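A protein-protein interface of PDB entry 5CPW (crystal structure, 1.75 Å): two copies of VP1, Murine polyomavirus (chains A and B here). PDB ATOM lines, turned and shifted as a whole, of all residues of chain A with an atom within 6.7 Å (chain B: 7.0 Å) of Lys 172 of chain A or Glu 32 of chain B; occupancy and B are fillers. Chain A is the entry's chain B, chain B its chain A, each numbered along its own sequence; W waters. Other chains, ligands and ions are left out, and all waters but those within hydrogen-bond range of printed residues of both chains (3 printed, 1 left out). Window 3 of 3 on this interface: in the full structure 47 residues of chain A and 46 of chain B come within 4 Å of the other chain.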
ATOM      1  N   GLY A 144      34.322   1.260 -22.180  1.00  0.00           N
ATOM      2  CA  GLY A 144      33.604   2.230 -21.353  1.00  0.00           C
ATOM      3  C   GLY A 144      33.517   1.775 -19.904  1.00  0.00           C
ATOM      4  O   GLY A 144      33.364   0.585 -19.635  1.00  0.00           O
ATOM      5  N   LEU A 145      33.649   2.726 -18.978  1.00  0.00           N
ATOM      6  CA  LEU A 145      33.396   2.506 -17.553  1.00  0.00           C
ATOM      7  C   LEU A 145      33.257   3.868 -16.894  1.00  0.00           C
ATOM      8  O   LEU A 145      34.139   4.728 -17.034  1.00  0.00           O
ATOM      9  CB  LEU A 145      34.534   1.710 -16.881  1.00  0.00           C
ATOM     10  CG  LEU A 145      34.321   1.257 -15.423  1.00  0.00           C
ATOM     11  CD1 LEU A 145      35.136   0.004 -15.119  1.00  0.00           C
ATOM     12  CD2 LEU A 145      34.676   2.365 -14.426  1.00  0.00           C
ATOM     13  N   ALA A 149      26.329   5.721 -13.879  1.00  0.00           N
ATOM     14  CA  ALA A 149      25.576   5.383 -15.088  1.00  0.00           C
ATOM     15  C   ALA A 149      24.376   6.319 -15.272  1.00  0.00           C
ATOM     16  O   ALA A 149      23.726   6.304 -16.326  1.00  0.00           O
ATOM     17  CB  ALA A 149      25.113   3.927 -15.046  1.00  0.00           C
ATOM     18  N   MET A 169      22.822   4.241 -20.419  1.00  0.00           N
ATOM     19  CA  MET A 169      23.758   3.437 -19.638  1.00  0.00           C
ATOM     20  C   MET A 169      23.003   2.548 -18.637  1.00  0.00           C
ATOM     21  O   MET A 169      21.893   2.872 -18.219  1.00  0.00           O
ATOM     22  CB  MET A 169      24.757   4.329 -18.910  1.00  0.00           C
ATOM     23  CG  MET A 169      25.840   4.914 -19.817  1.00  0.00           C
ATOM     24  SD  MET A 169      27.056   5.825 -18.856  1.00  0.00           S
ATOM     25  CE  MET A 169      26.143   7.310 -18.436  1.00  0.00           C
ATOM     26  N   VAL A 170      23.616   1.422 -18.278  1.00  0.00           N
ATOM     27  CA  VAL A 170      23.038   0.469 -17.325  1.00  0.00           C
ATOM     28  C   VAL A 170      23.977   0.388 -16.123  1.00  0.00           C
ATOM     29  O   VAL A 170      25.112   0.860 -16.203  1.00  0.00           O
ATOM     30  CB  VAL A 170      22.835  -0.933 -17.951  1.00  0.00           C
ATOM     31  CG1 VAL A 170      21.774  -0.881 -19.047  1.00  0.00           C
ATOM     32  CG2 VAL A 170      24.146  -1.491 -18.505  1.00  0.00           C
ATOM     33  N   ASN A 171      23.524  -0.222 -15.028  1.00  0.00           N
ATOM     34  CA  ASN A 171      24.359  -0.267 -13.826  1.00  0.00           C
ATOM     35  C   ASN A 171      25.709  -0.957 -14.038  1.00  0.00           C
ATOM     36  O   ASN A 171      26.700  -0.557 -13.431  1.00  0.00           O
ATOM     37  CB  ASN A 171      23.588  -0.771 -12.581  1.00  0.00           C
ATOM     38  CG  ASN A 171      23.417  -2.285 -12.530  1.00  0.00           C
ATOM     39  OD1 ASN A 171      23.290  -2.969 -13.552  1.00  0.00           O
ATOM     40  ND2 ASN A 171      23.377  -2.820 -11.301  1.00  0.00           N
ATOM     41  N   LYS A 172      25.744  -1.954 -14.930  1.00  0.00           N
ATOM     42  CA  LYS A 172      26.984  -2.668 -15.293  1.00  0.00           C
ATOM     43  C   LYS A 172      28.047  -1.739 -15.865  1.00  0.00           C
ATOM     44  O   LYS A 172      29.224  -2.086 -15.881  1.00  0.00           O
ATOM     45  CB  LYS A 172      26.711  -3.750 -16.348  1.00  0.00           C
ATOM     46  CG  LYS A 172      25.803  -4.887 -15.934  1.00  0.00           C
ATOM     47  CD  LYS A 172      25.752  -5.921 -17.055  1.00  0.00           C
ATOM     48  CE  LYS A 172      24.532  -6.819 -16.946  1.00  0.00           C
ATOM     49  NZ  LYS A 172      23.294  -6.113 -17.373  1.00  0.00           N
ATOM     50  N   ASP A 173      27.637  -0.569 -16.355  1.00  0.00           N
ATOM     51  CA  ASP A 173      28.596   0.405 -16.906  1.00  0.00           C
ATOM     52  C   ASP A 173      29.463   1.092 -15.839  1.00  0.00           C
ATOM     53  O   ASP A 173      30.430   1.791 -16.162  1.00  0.00           O
ATOM     54  CB  ASP A 173      27.868   1.435 -17.786  1.00  0.00           C
ATOM     55  CG  ASP A 173      27.327   0.821 -19.081  1.00  0.00           C
ATOM     56  OD1 ASP A 173      27.956  -0.121 -19.623  1.00  0.00           O
ATOM     57  OD2 ASP A 173      26.268   1.275 -19.551  1.00  0.00           O
ATOM     58  N   GLN A 174      29.125   0.876 -14.569  1.00  0.00           N
ATOM     59  CA  GLN A 174      29.959   1.347 -13.453  1.00  0.00           C
ATOM     60  C   GLN A 174      31.040   0.334 -13.088  1.00  0.00           C
ATOM     61  O   GLN A 174      31.927   0.622 -12.275  1.00  0.00           O
ATOM     62  CB  GLN A 174      29.093   1.708 -12.241  1.00  0.00           C
ATOM     63  CG  GLN A 174      28.095   2.819 -12.573  1.00  0.00           C
ATOM     64  CD  GLN A 174      27.183   3.220 -11.432  1.00  0.00           C
ATOM     65  OE1 GLN A 174      26.318   4.088 -11.607  1.00  0.00           O
ATOM     66  NE2 GLN A 174      27.356   2.600 -10.261  1.00  0.00           N
ATOM     67  N   VAL A 175      30.942  -0.856 -13.684  1.00  0.00           N
ATOM     68  CA  VAL A 175      32.007  -1.878 -13.633  1.00  0.00           C
ATOM     69  C   VAL A 175      32.370  -2.233 -15.086  1.00  0.00           C
ATOM     70  O   VAL A 175      32.271  -1.375 -15.963  1.00  0.00           O
ATOM     71  CB  VAL A 175      31.610  -3.123 -12.796  1.00  0.00           C
ATOM     72  CG1 VAL A 175      31.418  -2.743 -11.330  1.00  0.00           C
ATOM     73  CG2 VAL A 175      30.346  -3.788 -13.328  1.00  0.00           C
ATOM     74  N   LEU A 176      32.806  -3.466 -15.344  1.00  0.00           N
ATOM     75  CA  LEU A 176      33.161  -3.855 -16.722  1.00  0.00           C
ATOM     76  C   LEU A 176      31.946  -4.451 -17.435  1.00  0.00           C
ATOM     77  O   LEU A 176      31.498  -5.549 -17.096  1.00  0.00           O
ATOM     78  CB  LEU A 176      34.329  -4.863 -16.731  1.00  0.00           C
ATOM     79  CG  LEU A 176      35.189  -5.015 -18.005  1.00  0.00           C
ATOM     80  CD1 LEU A 176      34.398  -5.473 -19.232  1.00  0.00           C
ATOM     81  CD2 LEU A 176      35.945  -3.730 -18.296  1.00  0.00           C
ATOM     82  N   ASN A 177      31.418  -3.709 -18.413  1.00  0.00           N
ATOM     83  CA  ASN A 177      30.342  -4.183 -19.271  1.00  0.00           C
ATOM     84  C   ASN A 177      30.901  -4.324 -20.691  1.00  0.00           C
ATOM     85  O   ASN A 177      31.134  -3.309 -21.351  1.00  0.00           O
ATOM     86  CB  ASN A 177      29.167  -3.197 -19.259  1.00  0.00           C
ATOM     87  CG  ASN A 177      28.044  -3.603 -20.203  1.00  0.00           C
ATOM     88  OD1 ASN A 177      28.064  -4.693 -20.787  1.00  0.00           O
ATOM     89  ND2 ASN A 177      27.044  -2.730 -20.344  1.00  0.00           N
ATOM     90  N   PRO A 178      31.104  -5.574 -21.170  1.00  0.00           N
ATOM     91  CA  PRO A 178      31.733  -5.842 -22.477  1.00  0.00           C
ATOM     92  C   PRO A 178      30.990  -5.246 -23.676  1.00  0.00           C
ATOM     93  O   PRO A 178      31.565  -5.113 -24.753  1.00  0.00           O
ATOM     94  CB  PRO A 178      31.720  -7.371 -22.567  1.00  0.00           C
ATOM     95  CG  PRO A 178      31.655  -7.836 -21.159  1.00  0.00           C
ATOM     96  CD  PRO A 178      30.832  -6.818 -20.428  1.00  0.00           C
ATOM     97  N   ILE A 179      29.714  -4.913 -23.492  1.00  0.00           N
ATOM     98  CA  ILE A 179      28.916  -4.281 -24.549  1.00  0.00           C
ATOM     99  C   ILE A 179      29.397  -2.848 -24.825  1.00  0.00           C
ATOM    100  O   ILE A 179      29.295  -2.355 -25.946  1.00  0.00           O
ATOM    101  CB  ILE A 179      27.411  -4.270 -24.179  1.00  0.00           C
ATOM    102  CG1 ILE A 179      26.874  -5.705 -24.115  1.00  0.00           C
ATOM    103  CG2 ILE A 179      26.593  -3.442 -25.168  1.00  0.00           C
ATOM    104  CD1 ILE A 179      25.535  -5.835 -23.410  1.00  0.00           C
ATOM    105  N   SER A 180      29.935  -2.191 -23.801  1.00  0.00           N
ATOM    106  CA  SER A 180      30.289  -0.773 -23.903  1.00  0.00           C
ATOM    107  C   SER A 180      31.711  -0.586 -24.435  1.00  0.00           C
ATOM    108  O   SER A 180      32.647  -0.300 -23.682  1.00  0.00           O
ATOM    109  CB  SER A 180      30.089  -0.088 -22.546  1.00  0.00           C
ATOM    110  OG  SER A 180      28.728  -0.225 -22.146  1.00  0.00           O
ATOM    111  N   ASN B  22      34.727  -8.559 -12.074  1.00  0.00           N
ATOM    112  CA  ASN B  22      34.151  -7.326 -11.523  1.00  0.00           C
ATOM    113  C   ASN B  22      34.331  -7.245 -10.014  1.00  0.00           C
ATOM    114  O   ASN B  22      34.362  -8.283  -9.349  1.00  0.00           O
ATOM    115  CB  ASN B  22      32.673  -7.219 -11.912  1.00  0.00           C
ATOM    116  CG  ASN B  22      32.501  -6.670 -13.312  1.00  0.00           C
ATOM    117  OD1 ASN B  22      33.210  -5.747 -13.706  1.00  0.00           O
ATOM    118  ND2 ASN B  22      31.581  -7.241 -14.075  1.00  0.00           N
ATOM    119  N   PRO B  28      25.367  -5.915  -4.588  1.00  0.00           N
ATOM    120  CA  PRO B  28      25.431  -6.979  -5.609  1.00  0.00           C
ATOM    121  C   PRO B  28      25.078  -6.446  -7.004  1.00  0.00           C
ATOM    122  O   PRO B  28      24.566  -5.322  -7.112  1.00  0.00           O
ATOM    123  CB  PRO B  28      24.367  -7.990  -5.137  1.00  0.00           C
ATOM    124  CG  PRO B  28      24.146  -7.671  -3.692  1.00  0.00           C
ATOM    125  CD  PRO B  28      24.327  -6.182  -3.584  1.00  0.00           C
ATOM    126  N   PRO B  29      25.339  -7.238  -8.065  1.00  0.00           N
ATOM    127  CA  PRO B  29      24.998  -6.827  -9.436  1.00  0.00           C
ATOM    128  C   PRO B  29      23.507  -6.542  -9.668  1.00  0.00           C
ATOM    129  O   PRO B  29      23.164  -5.732 -10.534  1.00  0.00           O
ATOM    130  CB  PRO B  29      25.464  -8.015 -10.283  1.00  0.00           C
ATOM    131  CG  PRO B  29      26.570  -8.630  -9.478  1.00  0.00           C
ATOM    132  CD  PRO B  29      26.101  -8.505  -8.053  1.00  0.00           C
ATOM    133  N   THR B  30      22.631  -7.198  -8.909  1.00  0.00           N
ATOM    134  CA  THR B  30      21.187  -6.958  -9.009  1.00  0.00           C
ATOM    135  C   THR B  30      20.670  -6.419  -7.665  1.00  0.00           C
ATOM    136  O   THR B  30      21.283  -6.685  -6.635  1.00  0.00           O
ATOM    137  CB  THR B  30      20.418  -8.234  -9.421  1.00  0.00           C
ATOM    138  OG1 THR B  30      20.536  -9.213  -8.389  1.00  0.00           O
ATOM    139  CG2 THR B  30      20.988  -8.808 -10.716  1.00  0.00           C
ATOM    140  N   PRO B  31      19.566  -5.642  -7.667  1.00  0.00           N
ATOM    141  CA  PRO B  31      18.739  -5.232  -8.814  1.00  0.00           C
ATOM    142  C   PRO B  31      19.501  -4.310  -9.764  1.00  0.00           C
ATOM    143  O   PRO B  31      20.334  -3.518  -9.328  1.00  0.00           O
ATOM    144  CB  PRO B  31      17.565  -4.487  -8.171  1.00  0.00           C
ATOM    145  CG  PRO B  31      18.055  -4.038  -6.845  1.00  0.00           C
ATOM    146  CD  PRO B  31      19.155  -4.973  -6.415  1.00  0.00           C
ATOM    147  N   GLU B  32      19.219  -4.426 -11.058  1.00  0.00           N
ATOM    148  CA  GLU B  32      19.887  -3.592 -12.057  1.00  0.00           C
ATOM    149  C   GLU B  32      19.388  -2.146 -12.031  1.00  0.00           C
ATOM    150  O   GLU B  32      20.117  -1.237 -12.417  1.00  0.00           O
ATOM    151  CB  GLU B  32      19.743  -4.210 -13.456  1.00  0.00           C
ATOM    152  CG  GLU B  32      20.441  -5.565 -13.553  1.00  0.00           C
ATOM    153  CD  GLU B  32      20.429  -6.182 -14.943  1.00  0.00           C
ATOM    154  OE1 GLU B  32      19.526  -5.866 -15.747  1.00  0.00           O
ATOM    155  OE2 GLU B  32      21.335  -6.999 -15.222  1.00  0.00           O
ATOM    156  N   SER B  33      18.156  -1.950 -11.557  1.00  0.00           N
ATOM    157  CA  SER B  33      17.504  -0.641 -11.529  1.00  0.00           C
ATOM    158  C   SER B  33      18.393   0.445 -10.937  1.00  0.00           C
ATOM    159  O   SER B  33      18.959   0.278  -9.856  1.00  0.00           O
ATOM    160  CB  SER B  33      16.202  -0.701 -10.734  1.00  0.00           C
ATOM    161  OG  SER B  33      15.750   0.608 -10.431  1.00  0.00           O
ATOM    162  N   LEU B  34      18.497   1.566 -11.645  1.00  0.00           N
ATOM    163  CA  LEU B  34      19.349   2.667 -11.191  1.00  0.00           C
ATOM    164  C   LEU B  34      18.693   3.532 -10.105  1.00  0.00           C
ATOM    165  O   LEU B  34      19.272   4.531  -9.673  1.00  0.00           O
ATOM    166  CB  LEU B  34      19.847   3.515 -12.381  1.00  0.00           C
ATOM    167  CG  LEU B  34      20.896   2.863 -13.298  1.00  0.00           C
ATOM    168  CD1 LEU B  34      21.133   3.696 -14.555  1.00  0.00           C
ATOM    169  CD2 LEU B  34      22.211   2.624 -12.560  1.00  0.00           C
ATOM    170  N   THR B  35      17.495   3.143  -9.666  1.00  0.00           N
ATOM    171  CA  THR B  35      16.851   3.774  -8.512  1.00  0.00           C
ATOM    172  C   THR B  35      16.690   2.812  -7.328  1.00  0.00           C
ATOM    173  O   THR B  35      16.579   3.253  -6.182  1.00  0.00           O
ATOM    174  CB  THR B  35      15.471   4.385  -8.853  1.00  0.00           C
ATOM    175  OG1 THR B  35      14.566   3.357  -9.292  1.00  0.00           O
ATOM    176  CG2 THR B  35      15.598   5.455  -9.932  1.00  0.00           C
ATOM    177  N   GLU B  36      16.691   1.509  -7.605  1.00  0.00           N
ATOM    178  CA  GLU B  36      16.389   0.504  -6.580  1.00  0.00           C
ATOM    179  C   GLU B  36      17.642  -0.115  -5.943  1.00  0.00           C
ATOM    180  O   GLU B  36      17.557  -1.155  -5.284  1.00  0.00           O
ATOM    181  CB  GLU B  36      15.469  -0.596  -7.147  1.00  0.00           C
ATOM    182  CG  GLU B  36      14.086  -0.119  -7.592  1.00  0.00           C
ATOM    183  CD  GLU B  36      13.130   0.131  -6.435  1.00  0.00           C
ATOM    184  OE1 GLU B  36      11.946   0.440  -6.700  1.00  0.00           O
ATOM    185  OE2 GLU B  36      13.558   0.023  -5.263  1.00  0.00           O
ATOM    186  N   GLY B  37      18.797   0.527  -6.121  1.00  0.00           N
ATOM    187  CA  GLY B  37      20.033   0.023  -5.534  1.00  0.00           C
ATOM    188  C   GLY B  37      21.147  -0.205  -6.535  1.00  0.00           C
ATOM    189  O   GLY B  37      22.314  -0.167  -6.173  1.00  0.00           O
ATOM    190  N   GLY B  38      20.789  -0.442  -7.799  1.00  0.00           N
ATOM    191  CA  GLY B  38      21.786  -0.693  -8.855  1.00  0.00           C
ATOM    192  C   GLY B  38      22.740   0.464  -9.092  1.00  0.00           C
ATOM    193  O   GLY B  38      23.868   0.264  -9.533  1.00  0.00           O
ATOM    194  N   GLN B  39      22.298   1.681  -8.769  1.00  0.00           N
ATOM    195  CA  GLN B  39      23.185   2.853  -8.789  1.00  0.00           C
ATOM    196  C   GLN B  39      24.443   2.709  -7.895  1.00  0.00           C
ATOM    197  O   GLN B  39      25.426   3.429  -8.086  1.00  0.00           O
ATOM    198  CB  GLN B  39      22.404   4.144  -8.458  1.00  0.00           C
ATOM    199  CG  GLN B  39      21.896   4.288  -7.016  1.00  0.00           C
ATOM    200  CD  GLN B  39      20.487   3.759  -6.811  1.00  0.00           C
ATOM    201  OE1 GLN B  39      20.143   2.674  -7.275  1.00  0.00           O
ATOM    202  NE2 GLN B  39      19.656   4.532  -6.108  1.00  0.00           N
ATOM    203  N   TYR B  41      26.129  -0.236  -7.680  1.00  0.00           N
ATOM    204  CA  TYR B  41      26.958  -1.325  -8.198  1.00  0.00           C
ATOM    205  C   TYR B  41      28.351  -0.817  -8.618  1.00  0.00           C
ATOM    206  O   TYR B  41      28.481   0.150  -9.368  1.00  0.00           O
ATOM    207  CB  TYR B  41      26.226  -2.091  -9.325  1.00  0.00           C
ATOM    208  CG  TYR B  41      26.953  -3.323  -9.823  1.00  0.00           C
ATOM    209  CD1 TYR B  41      27.616  -4.180  -8.934  1.00  0.00           C
ATOM    210  CD2 TYR B  41      26.961  -3.647 -11.180  1.00  0.00           C
ATOM    211  CE1 TYR B  41      28.291  -5.302  -9.389  1.00  0.00           C
ATOM    212  CE2 TYR B  41      27.609  -4.780 -11.645  1.00  0.00           C
ATOM    213  CZ  TYR B  41      28.281  -5.602 -10.744  1.00  0.00           C
ATOM    214  OH  TYR B  41      28.938  -6.724 -11.207  1.00  0.00           O
HETATM  215  O   HOH W   1      25.521   5.946  -9.217  1.00  0.00           O
HETATM  216  O   HOH W   2      29.172  -6.728 -16.295  1.00  0.00           O
HETATM  217  O   HOH W   3      20.744  -0.994 -15.105  1.00  0.00           O
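The backbone NH (N) of Leu 176 of chain A is in hydrogen-bond range of the side-chain amide oxygen (OD1) of Asn 22 of chain B, 2.8 Å away.
O of Gln 39 of chain B lies within hydrogen-bond range of NE2 of Gln 174 of chain A.
The backbone carbonyl oxygen (O) of Pro 29 of chain B is in hydrogen-bond range of the side-chain amide nitrogen (ND2) of Asn 171 of chain A.
The side-chain carboxylate (OE2) of Glu 32 of chain B lies within salt-bridge range of the side-chain amino group (NZ) of Lys 172 of chain A, at 3.0 Å.
The side-chain amide nitrogen (NE2) of Gln 174 of chain A lies within hydrogen-bond range of the backbone carbonyl oxygen (O) of Tyr 41 of chain B, at 2.8 Å.
O of Leu 34 of chain B lies close to OE1 of Gln 39 of chain B (3.2 Å).
The backbone NH (N) of Gly 37 of chain B sits at hydrogen-bond distance from the side-chain amide oxygen (OE1) of Gln 39 of chain B (2.8 Å).
O of Ser 33 of chain B lies within hydrogen-bond range of N of Gly 38 of chain B (2.8 Å).
O of Pro 31 of chain B lies close to N of Gly 38 of chain B.
The side-chain amide nitrogen (NE2) of Gln 39 of chain B sits at hydrogen-bond distance from the backbone carbonyl oxygen (O) of Thr 35 of chain B, 3.3 Å away.
The backbone NH of Ala 149 of chain A is in hydrogen-bond range of the side-chain amide oxygen of Gln 174 of chain A (2.8 Å).
Leu 34 of chain B touches Met 169 of chain A.
Asn 171 of chain A touches Pro 31 of chain B.
Asn 171 of chain A touches Glu 32 of chain B.
CB of Asn 171 of chain A touches CD2 of Leu 34 of chain B (3.7 Å).
Asn 171 of chain A touches Gly 38 of chain B (CB to O, 3.2 Å).
CB of Tyr 41 of chain B touches ND2 of Asn 171 of chain A (3.5 Å).
Asn 22 of chain B touches Val 175 of chain A.
Val 175 of chain A touches Tyr 41 of chain B.
Lys 172 of chain A touches just one residue of chain B: Glu 32.
Of the printed residues of chain A, Glu 32 of chain B touches Asn 171 (3.5 Å) and Lys 172 (3.0 Å).
Of the printed residues of chain B, Gln 174 of chain A touches Gln 39 (3.0 Å) and Tyr 41 (2.8 Å).
Of the printed residues of chain B, Met 169 of chain A touches Leu 34.
Of the printed residues of chain A, Tyr 41 of chain B touches Asn 171, Gln 174 and Val 175.
Of the printed residues of chain A, Asn 22 of chain B touches Val 175 and Leu 176.
The nearest residue of chain B that does not touch Lys 172 of chain A is Tyr 41 of chain B (4.2 Å).
The nearest residue of chain A that does not touch Glu 32 of chain B is Val 170 of chain A (5.6 Å).
Hydrophobic or aromatic side chains of chain B within 4 Å of the printed part of chain A: Leu 34 and Tyr 41.
Among the printed residues, 13 pairs touch across the chains.
No position is printed for both chains.
Of the 13 pairs that touch across the chains among the printed residues, none has its exchanged pair printed and touching as well.
Water W2 bridges O of Leu 176 of chain A (2.7 Å) and ND2 of Asn 22 of chain B (3.3 Å).
Water W1 bridges O of Gln 39 of chain B (2.8 Å) and OE1 of Gln 174 of chain A (3.1 Å).
Water W3 bridges the backbone carbonyl oxygen of Glu 32 of chain B (2.8 Å) and the backbone NH of Asn 171 of chain A (2.9 Å).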
